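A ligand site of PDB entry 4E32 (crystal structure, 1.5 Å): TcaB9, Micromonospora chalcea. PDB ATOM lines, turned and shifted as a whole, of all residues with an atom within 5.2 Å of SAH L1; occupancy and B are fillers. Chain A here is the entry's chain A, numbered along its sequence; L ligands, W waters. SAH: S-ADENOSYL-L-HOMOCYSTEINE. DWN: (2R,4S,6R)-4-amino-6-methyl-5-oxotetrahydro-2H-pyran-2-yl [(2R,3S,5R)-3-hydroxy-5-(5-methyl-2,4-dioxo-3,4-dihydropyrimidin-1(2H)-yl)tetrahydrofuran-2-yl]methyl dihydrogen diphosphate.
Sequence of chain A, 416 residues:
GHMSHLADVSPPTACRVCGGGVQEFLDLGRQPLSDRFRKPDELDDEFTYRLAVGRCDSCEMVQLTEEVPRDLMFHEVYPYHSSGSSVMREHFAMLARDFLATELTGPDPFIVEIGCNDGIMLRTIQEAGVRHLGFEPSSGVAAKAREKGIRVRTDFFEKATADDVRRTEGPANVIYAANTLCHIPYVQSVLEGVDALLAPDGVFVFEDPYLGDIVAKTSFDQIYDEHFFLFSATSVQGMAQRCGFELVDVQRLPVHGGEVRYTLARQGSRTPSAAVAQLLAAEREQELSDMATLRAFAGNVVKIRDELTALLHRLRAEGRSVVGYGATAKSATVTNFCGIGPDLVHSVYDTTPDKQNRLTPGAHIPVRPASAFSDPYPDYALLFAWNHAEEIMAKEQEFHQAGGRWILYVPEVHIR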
ATOM      1  N   ARG A  70     -12.554 -12.080 -26.019  1.00  0.00           N
ATOM      2  CA  ARG A  70     -12.931 -13.486 -25.877  1.00  0.00           C
ATOM      3  C   ARG A  70     -11.803 -14.365 -25.356  1.00  0.00           C
ATOM      4  O   ARG A  70     -12.023 -15.326 -24.608  1.00  0.00           O
ATOM      5  CB  ARG A  70     -13.536 -14.041 -27.182  1.00  0.00           C
ATOM      6  CG  ARG A  70     -12.484 -14.075 -28.335  1.00  0.00           C
ATOM      7  CD  ARG A  70     -13.154 -14.485 -29.645  1.00  0.00           C
ATOM      8  NE  ARG A  70     -12.192 -14.515 -30.731  1.00  0.00           N
ATOM      9  CZ  ARG A  70     -12.565 -14.866 -31.951  1.00  0.00           C
ATOM     10  NH1 ARG A  70     -13.824 -15.248 -32.168  1.00  0.00           N
ATOM     11  NH2 ARG A  70     -11.675 -14.859 -32.937  1.00  0.00           N
ATOM     12  N   PHE A  74     -12.104 -17.516 -22.545  1.00  0.00           N
ATOM     13  CA  PHE A  74     -12.243 -18.825 -23.158  1.00  0.00           C
ATOM     14  C   PHE A  74     -10.865 -19.182 -23.734  1.00  0.00           C
ATOM     15  O   PHE A  74     -10.384 -18.479 -24.611  1.00  0.00           O
ATOM     16  CB  PHE A  74     -13.331 -18.775 -24.235  1.00  0.00           C
ATOM     17  CG  PHE A  74     -14.621 -18.144 -23.767  1.00  0.00           C
ATOM     18  CD1 PHE A  74     -15.303 -18.771 -22.736  1.00  0.00           C
ATOM     19  CD2 PHE A  74     -15.134 -17.028 -24.421  1.00  0.00           C
ATOM     20  CE1 PHE A  74     -16.477 -18.197 -22.291  1.00  0.00           C
ATOM     21  CE2 PHE A  74     -16.322 -16.443 -23.976  1.00  0.00           C
ATOM     22  CZ  PHE A  74     -16.962 -17.082 -22.941  1.00  0.00           C
ATOM     23  N   TYR A  78     -10.060 -22.896 -19.321  1.00  0.00           N
ATOM     24  CA  TYR A  78     -11.423 -22.594 -18.897  1.00  0.00           C
ATOM     25  C   TYR A  78     -11.956 -23.725 -18.040  1.00  0.00           C
ATOM     26  O   TYR A  78     -11.900 -24.892 -18.404  1.00  0.00           O
ATOM     27  CB  TYR A  78     -12.304 -22.516 -20.130  1.00  0.00           C
ATOM     28  CG  TYR A  78     -13.730 -22.075 -19.889  1.00  0.00           C
ATOM     29  CD1 TYR A  78     -14.796 -22.962 -20.072  1.00  0.00           C
ATOM     30  CD2 TYR A  78     -13.996 -20.744 -19.557  1.00  0.00           C
ATOM     31  CE1 TYR A  78     -16.119 -22.554 -19.902  1.00  0.00           C
ATOM     32  CE2 TYR A  78     -15.334 -20.320 -19.372  1.00  0.00           C
ATOM     33  CZ  TYR A  78     -16.370 -21.234 -19.572  1.00  0.00           C
ATOM     34  OH  TYR A  78     -17.682 -20.831 -19.423  1.00  0.00           O
ATOM     35  N   TYR A  80     -15.136 -24.500 -16.620  1.00  0.00           N
ATOM     36  CA  TYR A  80     -16.487 -25.021 -16.326  1.00  0.00           C
ATOM     37  C   TYR A  80     -16.706 -26.331 -17.056  1.00  0.00           C
ATOM     38  O   TYR A  80     -16.458 -26.419 -18.269  1.00  0.00           O
ATOM     39  CB  TYR A  80     -17.538 -24.068 -16.895  1.00  0.00           C
ATOM     40  CG  TYR A  80     -18.937 -24.586 -16.654  1.00  0.00           C
ATOM     41  CD1 TYR A  80     -19.450 -24.641 -15.361  1.00  0.00           C
ATOM     42  CD2 TYR A  80     -19.751 -24.891 -17.756  1.00  0.00           C
ATOM     43  CE1 TYR A  80     -20.747 -25.070 -15.145  1.00  0.00           C
ATOM     44  CE2 TYR A  80     -21.051 -25.334 -17.530  1.00  0.00           C
ATOM     45  CZ  TYR A  80     -21.508 -25.401 -16.230  1.00  0.00           C
ATOM     46  OH  TYR A  80     -22.811 -25.790 -16.012  1.00  0.00           O
ATOM     47  N   SER A  82     -19.528 -28.876 -18.154  1.00  0.00           N
ATOM     48  CA  SER A  82     -20.996 -28.933 -18.186  1.00  0.00           C
ATOM     49  C   SER A  82     -21.477 -30.242 -17.565  1.00  0.00           C
ATOM     50  O   SER A  82     -22.557 -30.267 -16.950  1.00  0.00           O
ATOM     51  CB  SER A  82     -21.435 -28.953 -19.653  1.00  0.00           C
ATOM     52  OG  SER A  82     -20.981 -27.739 -20.266  1.00  0.00           O
ATOM     53  N   PHE A  92     -29.638 -32.339 -21.723  1.00  0.00           N
ATOM     54  CA  PHE A  92     -29.049 -32.316 -23.055  1.00  0.00           C
ATOM     55  C   PHE A  92     -29.243 -33.600 -23.849  1.00  0.00           C
ATOM     56  O   PHE A  92     -29.463 -33.554 -25.053  1.00  0.00           O
ATOM     57  CB  PHE A  92     -27.584 -31.878 -23.024  1.00  0.00           C
ATOM     58  CG  PHE A  92     -27.436 -30.418 -22.683  1.00  0.00           C
ATOM     59  CD1 PHE A  92     -27.943 -29.446 -23.543  1.00  0.00           C
ATOM     60  CD2 PHE A  92     -26.765 -30.043 -21.522  1.00  0.00           C
ATOM     61  CE1 PHE A  92     -27.796 -28.112 -23.271  1.00  0.00           C
ATOM     62  CE2 PHE A  92     -26.616 -28.707 -21.263  1.00  0.00           C
ATOM     63  CZ  PHE A  92     -27.098 -27.730 -22.140  1.00  0.00           C
ATOM     64  N   GLU A 113     -22.553 -28.163 -33.083  1.00  0.00           N
ATOM     65  CA  GLU A 113     -22.830 -27.475 -31.836  1.00  0.00           C
ATOM     66  C   GLU A 113     -21.759 -26.410 -31.584  1.00  0.00           C
ATOM     67  O   GLU A 113     -20.557 -26.670 -31.679  1.00  0.00           O
ATOM     68  CB  GLU A 113     -22.936 -28.472 -30.662  1.00  0.00           C
ATOM     69  CG  GLU A 113     -23.183 -27.727 -29.357  1.00  0.00           C
ATOM     70  CD  GLU A 113     -23.368 -28.598 -28.144  1.00  0.00           C
ATOM     71  OE1 GLU A 113     -23.981 -28.166 -27.146  1.00  0.00           O
ATOM     72  OE2 GLU A 113     -22.883 -29.744 -28.109  1.00  0.00           O
ATOM     73  N   ILE A 114     -22.251 -25.229 -31.228  1.00  0.00           N
ATOM     74  CA  ILE A 114     -21.426 -24.089 -30.816  1.00  0.00           C
ATOM     75  C   ILE A 114     -21.336 -24.150 -29.306  1.00  0.00           C
ATOM     76  O   ILE A 114     -22.362 -24.007 -28.625  1.00  0.00           O
ATOM     77  CB  ILE A 114     -22.092 -22.755 -31.266  1.00  0.00           C
ATOM     78  CG1 ILE A 114     -22.326 -22.829 -32.770  1.00  0.00           C
ATOM     79  CG2 ILE A 114     -21.217 -21.557 -30.839  1.00  0.00           C
ATOM     80  CD1 ILE A 114     -23.038 -21.642 -33.413  1.00  0.00           C
ATOM     81  N   GLY A 115     -20.135 -24.360 -28.782  1.00  0.00           N
ATOM     82  CA  GLY A 115     -19.861 -24.319 -27.354  1.00  0.00           C
ATOM     83  C   GLY A 115     -20.120 -25.688 -26.745  1.00  0.00           C
ATOM     84  O   GLY A 115     -20.731 -25.765 -25.690  1.00  0.00           O
ATOM     85  N   CYS A 116     -19.634 -26.756 -27.385  1.00  0.00           N
ATOM     86  CA  CYS A 116     -19.980 -28.115 -26.937  1.00  0.00           C
ATOM     87  C   CYS A 116     -19.351 -28.484 -25.608  1.00  0.00           C
ATOM     88  O   CYS A 116     -19.748 -29.469 -24.964  1.00  0.00           O
ATOM     89  CB  CYS A 116     -19.638 -29.141 -28.029  1.00  0.00           C
ATOM     90  SG  CYS A 116     -17.853 -29.332 -28.291  1.00  0.00           S
ATOM     91  N   ASN A 117     -18.389 -27.723 -25.090  1.00  0.00           N
ATOM     92  CA  ASN A 117     -17.756 -27.989 -23.801  1.00  0.00           C
ATOM     93  C   ASN A 117     -17.226 -29.422 -23.770  1.00  0.00           C
ATOM     94  O   ASN A 117     -16.615 -29.915 -24.732  1.00  0.00           O
ATOM     95  CB  ASN A 117     -18.756 -27.585 -22.679  1.00  0.00           C
ATOM     96  CG  ASN A 117     -18.129 -27.455 -21.284  1.00  0.00           C
ATOM     97  OD1 ASN A 117     -18.073 -28.404 -20.506  1.00  0.00           O
ATOM     98  ND2 ASN A 117     -17.609 -26.250 -20.963  1.00  0.00           N
ATOM     99  N   ILE A 120     -21.300 -32.805 -23.400  1.00  0.00           N
ATOM    100  CA  ILE A 120     -22.567 -33.121 -22.736  1.00  0.00           C
ATOM    101  C   ILE A 120     -23.759 -33.385 -23.667  1.00  0.00           C
ATOM    102  O   ILE A 120     -24.567 -34.298 -23.426  1.00  0.00           O
ATOM    103  CB  ILE A 120     -22.895 -32.047 -21.667  1.00  0.00           C
ATOM    104  CG1 ILE A 120     -24.027 -32.514 -20.736  1.00  0.00           C
ATOM    105  CG2 ILE A 120     -23.211 -30.706 -22.319  1.00  0.00           C
ATOM    106  CD1 ILE A 120     -24.240 -31.626 -19.508  1.00  0.00           C
ATOM    107  N   PHE A 135     -17.824 -27.011 -31.898  1.00  0.00           N
ATOM    108  CA  PHE A 135     -16.871 -25.898 -31.789  1.00  0.00           C
ATOM    109  C   PHE A 135     -16.683 -25.643 -30.308  1.00  0.00           C
ATOM    110  O   PHE A 135     -17.645 -25.436 -29.555  1.00  0.00           O
ATOM    111  CB  PHE A 135     -17.413 -24.600 -32.389  1.00  0.00           C
ATOM    112  CG  PHE A 135     -17.217 -24.483 -33.878  1.00  0.00           C
ATOM    113  CD1 PHE A 135     -16.180 -23.734 -34.378  1.00  0.00           C
ATOM    114  CD2 PHE A 135     -18.058 -25.166 -34.755  1.00  0.00           C
ATOM    115  CE1 PHE A 135     -16.000 -23.622 -35.768  1.00  0.00           C
ATOM    116  CE2 PHE A 135     -17.881 -25.086 -36.139  1.00  0.00           C
ATOM    117  CZ  PHE A 135     -16.847 -24.283 -36.648  1.00  0.00           C
ATOM    118  N   GLU A 136     -15.426 -25.682 -29.894  1.00  0.00           N
ATOM    119  CA  GLU A 136     -15.139 -25.497 -28.464  1.00  0.00           C
ATOM    120  C   GLU A 136     -13.747 -24.878 -28.371  1.00  0.00           C
ATOM    121  O   GLU A 136     -12.740 -25.632 -28.425  1.00  0.00           O
ATOM    122  CB  GLU A 136     -15.240 -26.802 -27.663  1.00  0.00           C
ATOM    123  CG  GLU A 136     -15.056 -26.649 -26.142  1.00  0.00           C
ATOM    124  CD  GLU A 136     -15.670 -25.343 -25.665  1.00  0.00           C
ATOM    125  OE1 GLU A 136     -16.910 -25.358 -25.460  1.00  0.00           O
ATOM    126  OE2 GLU A 136     -14.941 -24.329 -25.531  1.00  0.00           O
ATOM    127  N   PRO A 137     -13.705 -23.547 -28.252  1.00  0.00           N
ATOM    128  CA  PRO A 137     -12.421 -22.840 -28.259  1.00  0.00           C
ATOM    129  C   PRO A 137     -11.616 -23.030 -26.987  1.00  0.00           C
ATOM    130  O   PRO A 137     -10.487 -22.549 -26.953  1.00  0.00           O
ATOM    131  CB  PRO A 137     -12.824 -21.379 -28.401  1.00  0.00           C
ATOM    132  CG  PRO A 137     -14.237 -21.322 -27.699  1.00  0.00           C
ATOM    133  CD  PRO A 137     -14.856 -22.609 -28.185  1.00  0.00           C
ATOM    134  N   SER A 138     -12.218 -23.617 -25.954  1.00  0.00           N
ATOM    135  CA  SER A 138     -11.551 -23.859 -24.683  1.00  0.00           C
ATOM    136  C   SER A 138     -10.982 -25.277 -24.752  1.00  0.00           C
ATOM    137  O   SER A 138     -11.718 -26.266 -24.621  1.00  0.00           O
ATOM    138  CB  SER A 138     -12.477 -23.665 -23.467  1.00  0.00           C
ATOM    139  OG  SER A 138     -12.830 -22.285 -23.413  1.00  0.00           O
ATOM    140  N   VAL A 141     -11.557 -28.427 -22.020  1.00  0.00           N
ATOM    141  CA  VAL A 141     -12.824 -29.159 -22.119  1.00  0.00           C
ATOM    142  C   VAL A 141     -13.059 -29.778 -23.507  1.00  0.00           C
ATOM    143  O   VAL A 141     -13.715 -30.820 -23.613  1.00  0.00           O
ATOM    144  CB  VAL A 141     -14.041 -28.304 -21.722  1.00  0.00           C
ATOM    145  CG1 VAL A 141     -13.959 -27.940 -20.262  1.00  0.00           C
ATOM    146  CG2 VAL A 141     -14.046 -27.036 -22.581  1.00  0.00           C
ATOM    147  N   ASP A 155     -11.913 -24.049 -31.779  1.00  0.00           N
ATOM    148  CA  ASP A 155     -11.933 -22.754 -32.457  1.00  0.00           C
ATOM    149  C   ASP A 155     -13.218 -22.078 -32.006  1.00  0.00           C
ATOM    150  O   ASP A 155     -14.203 -22.736 -31.622  1.00  0.00           O
ATOM    151  CB  ASP A 155     -12.125 -22.908 -33.973  1.00  0.00           C
ATOM    152  CG  ASP A 155     -10.825 -22.961 -34.730  1.00  0.00           C
ATOM    153  OD1 ASP A 155     -10.699 -23.942 -35.502  1.00  0.00           O
ATOM    154  OD2 ASP A 155      -9.985 -22.050 -34.515  1.00  0.00           O
ATOM    155  N   PHE A 156     -13.242 -20.756 -32.093  1.00  0.00           N
ATOM    156  CA  PHE A 156     -14.511 -20.054 -31.988  1.00  0.00           C
ATOM    157  C   PHE A 156     -15.332 -20.204 -33.260  1.00  0.00           C
ATOM    158  O   PHE A 156     -14.818 -20.091 -34.375  1.00  0.00           O
ATOM    159  CB  PHE A 156     -14.258 -18.559 -31.789  1.00  0.00           C
ATOM    160  CG  PHE A 156     -13.471 -18.242 -30.526  1.00  0.00           C
ATOM    161  CD1 PHE A 156     -14.169 -18.158 -29.327  1.00  0.00           C
ATOM    162  CD2 PHE A 156     -12.111 -18.003 -30.519  1.00  0.00           C
ATOM    163  CE1 PHE A 156     -13.512 -17.843 -28.095  1.00  0.00           C
ATOM    164  CE2 PHE A 156     -11.434 -17.697 -29.330  1.00  0.00           C
ATOM    165  CZ  PHE A 156     -12.148 -17.597 -28.116  1.00  0.00           C
ATOM    166  N   PHE A 157     -16.620 -20.436 -33.089  1.00  0.00           N
ATOM    167  CA  PHE A 157     -17.538 -20.283 -34.213  1.00  0.00           C
ATOM    168  C   PHE A 157     -17.676 -18.803 -34.517  1.00  0.00           C
ATOM    169  O   PHE A 157     -17.961 -18.008 -33.614  1.00  0.00           O
ATOM    170  CB  PHE A 157     -18.892 -20.906 -33.842  1.00  0.00           C
ATOM    171  CG  PHE A 157     -19.898 -20.938 -34.962  1.00  0.00           C
ATOM    172  CD1 PHE A 157     -20.620 -19.816 -35.349  1.00  0.00           C
ATOM    173  CD2 PHE A 157     -20.032 -22.114 -35.695  1.00  0.00           C
ATOM    174  CE1 PHE A 157     -21.523 -19.951 -36.432  1.00  0.00           C
ATOM    175  CE2 PHE A 157     -20.915 -22.232 -36.763  1.00  0.00           C
ATOM    176  CZ  PHE A 157     -21.667 -21.141 -37.149  1.00  0.00           C
ATOM    177  N   ALA A 178     -26.106 -23.951 -26.682  1.00  0.00           N
ATOM    178  CA  ALA A 178     -26.690 -23.716 -25.351  1.00  0.00           C
ATOM    179  C   ALA A 178     -25.763 -22.908 -24.443  1.00  0.00           C
ATOM    180  O   ALA A 178     -24.588 -23.295 -24.323  1.00  0.00           O
ATOM    181  CB  ALA A 178     -26.928 -25.058 -24.687  1.00  0.00           C
ATOM    182  N   ASN A 179     -26.284 -21.856 -23.820  1.00  0.00           N
ATOM    183  CA  ASN A 179     -25.488 -21.051 -22.855  1.00  0.00           C
ATOM    184  C   ASN A 179     -24.203 -20.614 -23.552  1.00  0.00           C
ATOM    185  O   ASN A 179     -23.143 -20.572 -22.923  1.00  0.00           O
ATOM    186  CB  ASN A 179     -25.160 -21.901 -21.619  1.00  0.00           C
ATOM    187  CG  ASN A 179     -26.473 -22.451 -21.044  1.00  0.00           C
ATOM    188  OD1 ASN A 179     -27.308 -21.586 -20.695  1.00  0.00           O
ATOM    189  ND2 ASN A 179     -26.699 -23.770 -20.964  1.00  0.00           N
ATOM    190  N   THR A 180     -24.304 -20.300 -24.837  1.00  0.00           N
ATOM    191  CA  THR A 180     -23.120 -19.843 -25.569  1.00  0.00           C
ATOM    192  C   THR A 180     -23.393 -18.634 -26.476  1.00  0.00           C
ATOM    193  O   THR A 180     -22.569 -17.702 -26.547  1.00  0.00           O
ATOM    194  CB  THR A 180     -22.581 -20.994 -26.458  1.00  0.00           C
ATOM    195  OG1 THR A 180     -22.199 -22.085 -25.613  1.00  0.00           O
ATOM    196  CG2 THR A 180     -21.318 -20.557 -27.151  1.00  0.00           C
ATOM    197  N   HIS A 183     -23.013 -15.332 -24.936  1.00  0.00           N
ATOM    198  CA  HIS A 183     -21.659 -15.008 -24.487  1.00  0.00           C
ATOM    199  C   HIS A 183     -20.910 -14.261 -25.586  1.00  0.00           C
ATOM    200  O   HIS A 183     -19.788 -13.793 -25.336  1.00  0.00           O
ATOM    201  CB  HIS A 183     -20.856 -16.309 -24.293  1.00  0.00           C
ATOM    202  CG  HIS A 183     -21.337 -17.152 -23.148  1.00  0.00           C
ATOM    203  ND1 HIS A 183     -22.669 -17.309 -22.826  1.00  0.00           N
ATOM    204  CD2 HIS A 183     -20.638 -17.896 -22.255  1.00  0.00           C
ATOM    205  CE1 HIS A 183     -22.755 -18.066 -21.744  1.00  0.00           C
ATOM    206  NE2 HIS A 183     -21.547 -18.468 -21.399  1.00  0.00           N
ATOM    207  N   ILE A 184     -21.488 -14.153 -26.780  1.00  0.00           N
ATOM    208  CA  ILE A 184     -20.734 -13.737 -27.954  1.00  0.00           C
ATOM    209  C   ILE A 184     -21.185 -12.356 -28.435  1.00  0.00           C
ATOM    210  O   ILE A 184     -22.255 -12.220 -29.036  1.00  0.00           O
ATOM    211  CB  ILE A 184     -20.909 -14.799 -29.058  1.00  0.00           C
ATOM    212  CG1 ILE A 184     -20.230 -16.125 -28.641  1.00  0.00           C
ATOM    213  CG2 ILE A 184     -20.242 -14.286 -30.372  1.00  0.00           C
ATOM    214  CD1 ILE A 184     -20.690 -17.282 -29.524  1.00  0.00           C
ATOM    215  N   TYR A 186     -19.993 -10.624 -30.792  1.00  0.00           N
ATOM    216  CA  TYR A 186     -19.893 -10.675 -32.266  1.00  0.00           C
ATOM    217  C   TYR A 186     -20.949 -11.572 -32.902  1.00  0.00           C
ATOM    218  O   TYR A 186     -20.719 -12.384 -33.819  1.00  0.00           O
ATOM    219  CB  TYR A 186     -18.477 -11.011 -32.764  1.00  0.00           C
ATOM    220  CG  TYR A 186     -17.878 -12.243 -32.101  1.00  0.00           C
ATOM    221  CD1 TYR A 186     -17.295 -12.172 -30.839  1.00  0.00           C
ATOM    222  CD2 TYR A 186     -17.910 -13.467 -32.769  1.00  0.00           C
ATOM    223  CE1 TYR A 186     -16.724 -13.315 -30.284  1.00  0.00           C
ATOM    224  CE2 TYR A 186     -17.355 -14.613 -32.202  1.00  0.00           C
ATOM    225  CZ  TYR A 186     -16.800 -14.531 -30.943  1.00  0.00           C
ATOM    226  OH  TYR A 186     -16.222 -15.646 -30.336  1.00  0.00           O
ATOM    227  N   HIS A 256     -30.803 -23.427 -15.403  1.00  0.00           N
ATOM    228  CA  HIS A 256     -30.019 -22.213 -15.247  1.00  0.00           C
ATOM    229  C   HIS A 256     -30.803 -20.961 -14.836  1.00  0.00           C
ATOM    230  O   HIS A 256     -30.489 -19.859 -15.287  1.00  0.00           O
ATOM    231  CB  HIS A 256     -29.229 -21.998 -16.524  1.00  0.00           C
ATOM    232  CG  HIS A 256     -28.096 -22.969 -16.662  1.00  0.00           C
ATOM    233  ND1 HIS A 256     -27.084 -23.072 -15.745  1.00  0.00           N
ATOM    234  CD2 HIS A 256     -27.847 -23.919 -17.603  1.00  0.00           C
ATOM    235  CE1 HIS A 256     -26.241 -24.022 -16.122  1.00  0.00           C
ATOM    236  NE2 HIS A 256     -26.705 -24.574 -17.238  1.00  0.00           N
HETATM  237  N   SAH L   1     -22.997 -25.627 -23.981  1.00  0.00           N
HETATM  238  CA  SAH L   1     -22.431 -25.918 -22.635  1.00  0.00           C
HETATM  239  CB  SAH L   1     -21.273 -25.016 -22.225  1.00  0.00           C
HETATM  240  CG  SAH L   1     -21.688 -23.567 -21.994  1.00  0.00           C
HETATM  241  SD  SAH L   1     -20.380 -22.582 -21.343  1.00  0.00           S
HETATM  242  C   SAH L   1     -23.562 -25.881 -21.652  1.00  0.00           C
HETATM  243  O   SAH L   1     -24.664 -25.424 -21.970  1.00  0.00           O
HETATM  244  OXT SAH L   1     -23.334 -26.294 -20.509  1.00  0.00           O
HETATM  245  C5' SAH L   1     -19.999 -21.563 -22.736  1.00  0.00           C
HETATM  246  C4' SAH L   1     -19.070 -22.276 -23.733  1.00  0.00           C
HETATM  247  O4' SAH L   1     -18.919 -21.500 -24.932  1.00  0.00           O
HETATM  248  C3' SAH L   1     -17.625 -22.527 -23.257  1.00  0.00           C
HETATM  249  O3' SAH L   1     -17.252 -23.920 -23.178  1.00  0.00           O
HETATM  250  C2' SAH L   1     -16.777 -21.649 -24.180  1.00  0.00           C
HETATM  251  O2' SAH L   1     -15.448 -22.085 -24.400  1.00  0.00           O
HETATM  252  C1' SAH L   1     -17.604 -21.767 -25.453  1.00  0.00           C
HETATM  253  N9  SAH L   1     -17.436 -20.624 -26.393  1.00  0.00           N
HETATM  254  C8  SAH L   1     -17.229 -19.314 -26.235  1.00  0.00           C
HETATM  255  N7  SAH L   1     -17.213 -18.574 -27.371  1.00  0.00           N
HETATM  256  C5  SAH L   1     -17.479 -19.499 -28.361  1.00  0.00           C
HETATM  257  C6  SAH L   1     -17.640 -19.437 -29.831  1.00  0.00           C
HETATM  258  N6  SAH L   1     -17.497 -18.300 -30.541  1.00  0.00           N
HETATM  259  N1  SAH L   1     -17.845 -20.642 -30.407  1.00  0.00           N
HETATM  260  C2  SAH L   1     -18.003 -21.799 -29.742  1.00  0.00           C
HETATM  261  N3  SAH L   1     -17.893 -21.947 -28.420  1.00  0.00           N
HETATM  262  C4  SAH L   1     -17.673 -20.820 -27.698  1.00  0.00           C
HETATM  263  O4  DWN L   2     -23.385 -19.709 -18.687  1.00  0.00           O
HETATM  264  C4  DWN L   2     -22.555 -20.476 -18.199  1.00  0.00           C
HETATM  265  C5  DWN L   2     -23.038 -21.719 -17.510  1.00  0.00           C
HETATM  266  C6  DWN L   2     -23.640 -22.797 -18.420  1.00  0.00           C
HETATM  267  O5  DWN L   2     -21.999 -22.439 -16.883  1.00  0.00           O
HETATM  268  C3  DWN L   2     -21.063 -20.308 -18.320  1.00  0.00           C
HETATM  269  N3  DWN L   2     -20.792 -18.973 -18.795  1.00  0.00           N
HETATM  270  C2  DWN L   2     -20.205 -20.774 -17.144  1.00  0.00           C
HETATM  271  C1  DWN L   2     -21.050 -21.628 -16.192  1.00  0.00           C
HETATM  272  O1  DWN L   2     -21.735 -20.742 -15.315  1.00  0.00           O
HETATM  273  P2  DWN L   2     -21.955 -21.190 -13.780  1.00  0.00           P
HETATM  274  O3P DWN L   2     -20.571 -21.466 -13.203  1.00  0.00           O
HETATM  275  O4P DWN L   2     -22.863 -20.174 -13.125  1.00  0.00           O
HETATM  276  OPP DWN L   2     -22.726 -22.588 -13.943  1.00  0.00           O
HETATM  277  P   DWN L   2     -23.423 -23.613 -12.889  1.00  0.00           P
HETATM  278  O1P DWN L   2     -23.824 -24.798 -13.747  1.00  0.00           O
HETATM  279  O2P DWN L   2     -24.517 -22.926 -12.157  1.00  0.00           O
HETATM  280  O5X DWN L   2     -22.174 -23.949 -11.952  1.00  0.00           O
HETATM  281  C5X DWN L   2     -22.403 -24.866 -10.884  1.00  0.00           C
HETATM  282  C4X DWN L   2     -21.111 -24.920 -10.082  1.00  0.00           C
HETATM  283  O4X DWN L   2     -21.484 -25.627  -8.905  1.00  0.00           O
HETATM  284  C3X DWN L   2     -20.052 -25.743 -10.810  1.00  0.00           C
HETATM  285  O3X DWN L   2     -18.779 -25.178 -10.455  1.00  0.00           O
HETATM  286  C2X DWN L   2     -20.230 -27.090 -10.166  1.00  0.00           C
HETATM  287  C1X DWN L   2     -20.768 -26.842  -8.764  1.00  0.00           C
HETATM  288  N11 DWN L   2     -21.726 -27.909  -8.441  1.00  0.00           N
HETATM  289  C21 DWN L   2     -21.499 -28.641  -7.341  1.00  0.00           C
HETATM  290  O21 DWN L   2     -20.550 -28.381  -6.589  1.00  0.00           O
HETATM  291  N31 DWN L   2     -22.361 -29.618  -6.964  1.00  0.00           N
HETATM  292  C61 DWN L   2     -22.755 -28.168  -9.274  1.00  0.00           C
HETATM  293  C51 DWN L   2     -23.645 -29.191  -9.002  1.00  0.00           C
HETATM  294  C5A DWN L   2     -24.800 -29.513  -9.910  1.00  0.00           C
HETATM  295  C41 DWN L   2     -23.378 -29.978  -7.768  1.00  0.00           C
HETATM  296  O41 DWN L   2     -24.141 -30.909  -7.413  1.00  0.00           O
HETATM  297  O   HOH W   1     -16.264 -15.955 -27.757  1.00  0.00           O
HETATM  298  O   HOH W   2     -24.315 -28.113 -24.566  1.00  0.00           O
HETATM  299  O   HOH W   3     -25.052 -26.593 -18.427  1.00  0.00           O
HETATM  300  O   HOH W   4     -23.851 -25.475 -26.780  1.00  0.00           O
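The side-chain carboxylate (OE2) of Glu 136 is in hydrogen-bond range of an oxygen (O2') of SAH L1 (2.6 Å). OXT of SAH L1 sits at hydrogen-bond distance from OG of Ser 82, 2.8 Å away. An oxygen (O2') of SAH L1 lies within hydrogen-bond range of the side-chain hydroxyl (OG) of Ser 138 (2.8 Å). ND2 of Asn 179 lies within hydrogen-bond range of O of SAH L1 (2.8 Å). The backbone NH (N) of Gly 115 sits close to a nitrogen (N3) of SAH L1, at 3.3 Å. N of SAH L1 sits at hydrogen-bond distance from O of Gly 115 (2.8 Å). O of Ala 178 is in hydrogen-bond range of N of SAH L1 (2.8 Å). A nitrogen (N6) of SAH L1 is in hydrogen-bond range of the side-chain hydroxyl (OH) of Tyr 186 (3.0 Å). A nitrogen (N1) of SAH L1 is in hydrogen-bond range of the backbone NH (N) of Phe 157 (3.0 Å). The backbone carbonyl oxygen (O) of Phe 157 lies within hydrogen-bond range of a nitrogen (N6) of SAH L1. ND2 of Asn 117 sits at hydrogen-bond distance from O3' of SAH L1 (3.2 Å). The side-chain hydroxyl of Thr 180 lies within hydrogen-bond range of an oxygen (O4') of SAH L1. OH of Tyr 78 sits close to SD of SAH L1 (3.7 Å). A ring nitrogen (NE2) of His 183 sits at hydrogen-bond distance from a nitrogen (N3) of DWN L2 (2.8 Å). An oxygen (O1P) of DWN L2 is in hydrogen-bond range of the side-chain hydroxyl of Tyr 80 (2.7 Å).
The side-chain carboxylate (OE1) of Glu 136 lies within hydrogen-bond range of the backbone NH (N) of Asn 117, 2.8 Å away. A ring nitrogen (NE2) of His 183 lies close to the backbone carbonyl oxygen (O) of Asn 179, 3.0 Å away. N of Gly 115 lies within hydrogen-bond range of O of Phe 135, at 2.8 Å. The side-chain hydroxyl (OG1) of Thr 180 sits at hydrogen-bond distance from the backbone carbonyl oxygen (O) of Ala 178 (3.0 Å). The side-chain hydroxyl (OH) of Tyr 186 is in hydrogen-bond range of the guanidinium group (NH1) of Arg 70 (3.0 Å). The side-chain amide nitrogen (ND2) of Asn 117 sits at hydrogen-bond distance from the backbone carbonyl oxygen (O) of Tyr 80 (2.9 Å). The backbone NH of Phe 135 lies within hydrogen-bond range of the backbone carbonyl oxygen of Glu 113 (2.8 Å). O of Phe 135 lies within hydrogen-bond range of N of Cys 116, at 3.2 Å.
Water W3 lies within hydrogen-bond range of OXT of SAH L1, NE2 of His 256 and OH of Tyr 80. Water W1 lies within hydrogen-bond range of the side-chain hydroxyl (OH) of Tyr 186 (2.6 Å) and a nitrogen (N7) of SAH L1 (2.8 Å). Water W2 bridges the side-chain carboxylate of Glu 113 (2.6 Å) and a nitrogen (N) of SAH L1 (2.9 Å).
Phe 74 touches SAH L1. Tyr 80 touches SAH L1. CZ of Phe 92 touches O of SAH L1, 3.4 Å away. Ile 114 touches SAH L1 (CG2 to C2, 3.4 Å). O of Phe 135 touches C2 of SAH L1, 3.7 Å away. Pro 137 touches SAH L1. CB of Phe 156 touches N6 of SAH L1, 3.5 Å away. His 183 touches SAH L1 (NE2 to C5', 3.7 Å). CD1 of Ile 184 touches N6 of SAH L1, 3.5 Å away. Of the 27 residues printed, 20 come within 4 Å of SAH L1.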
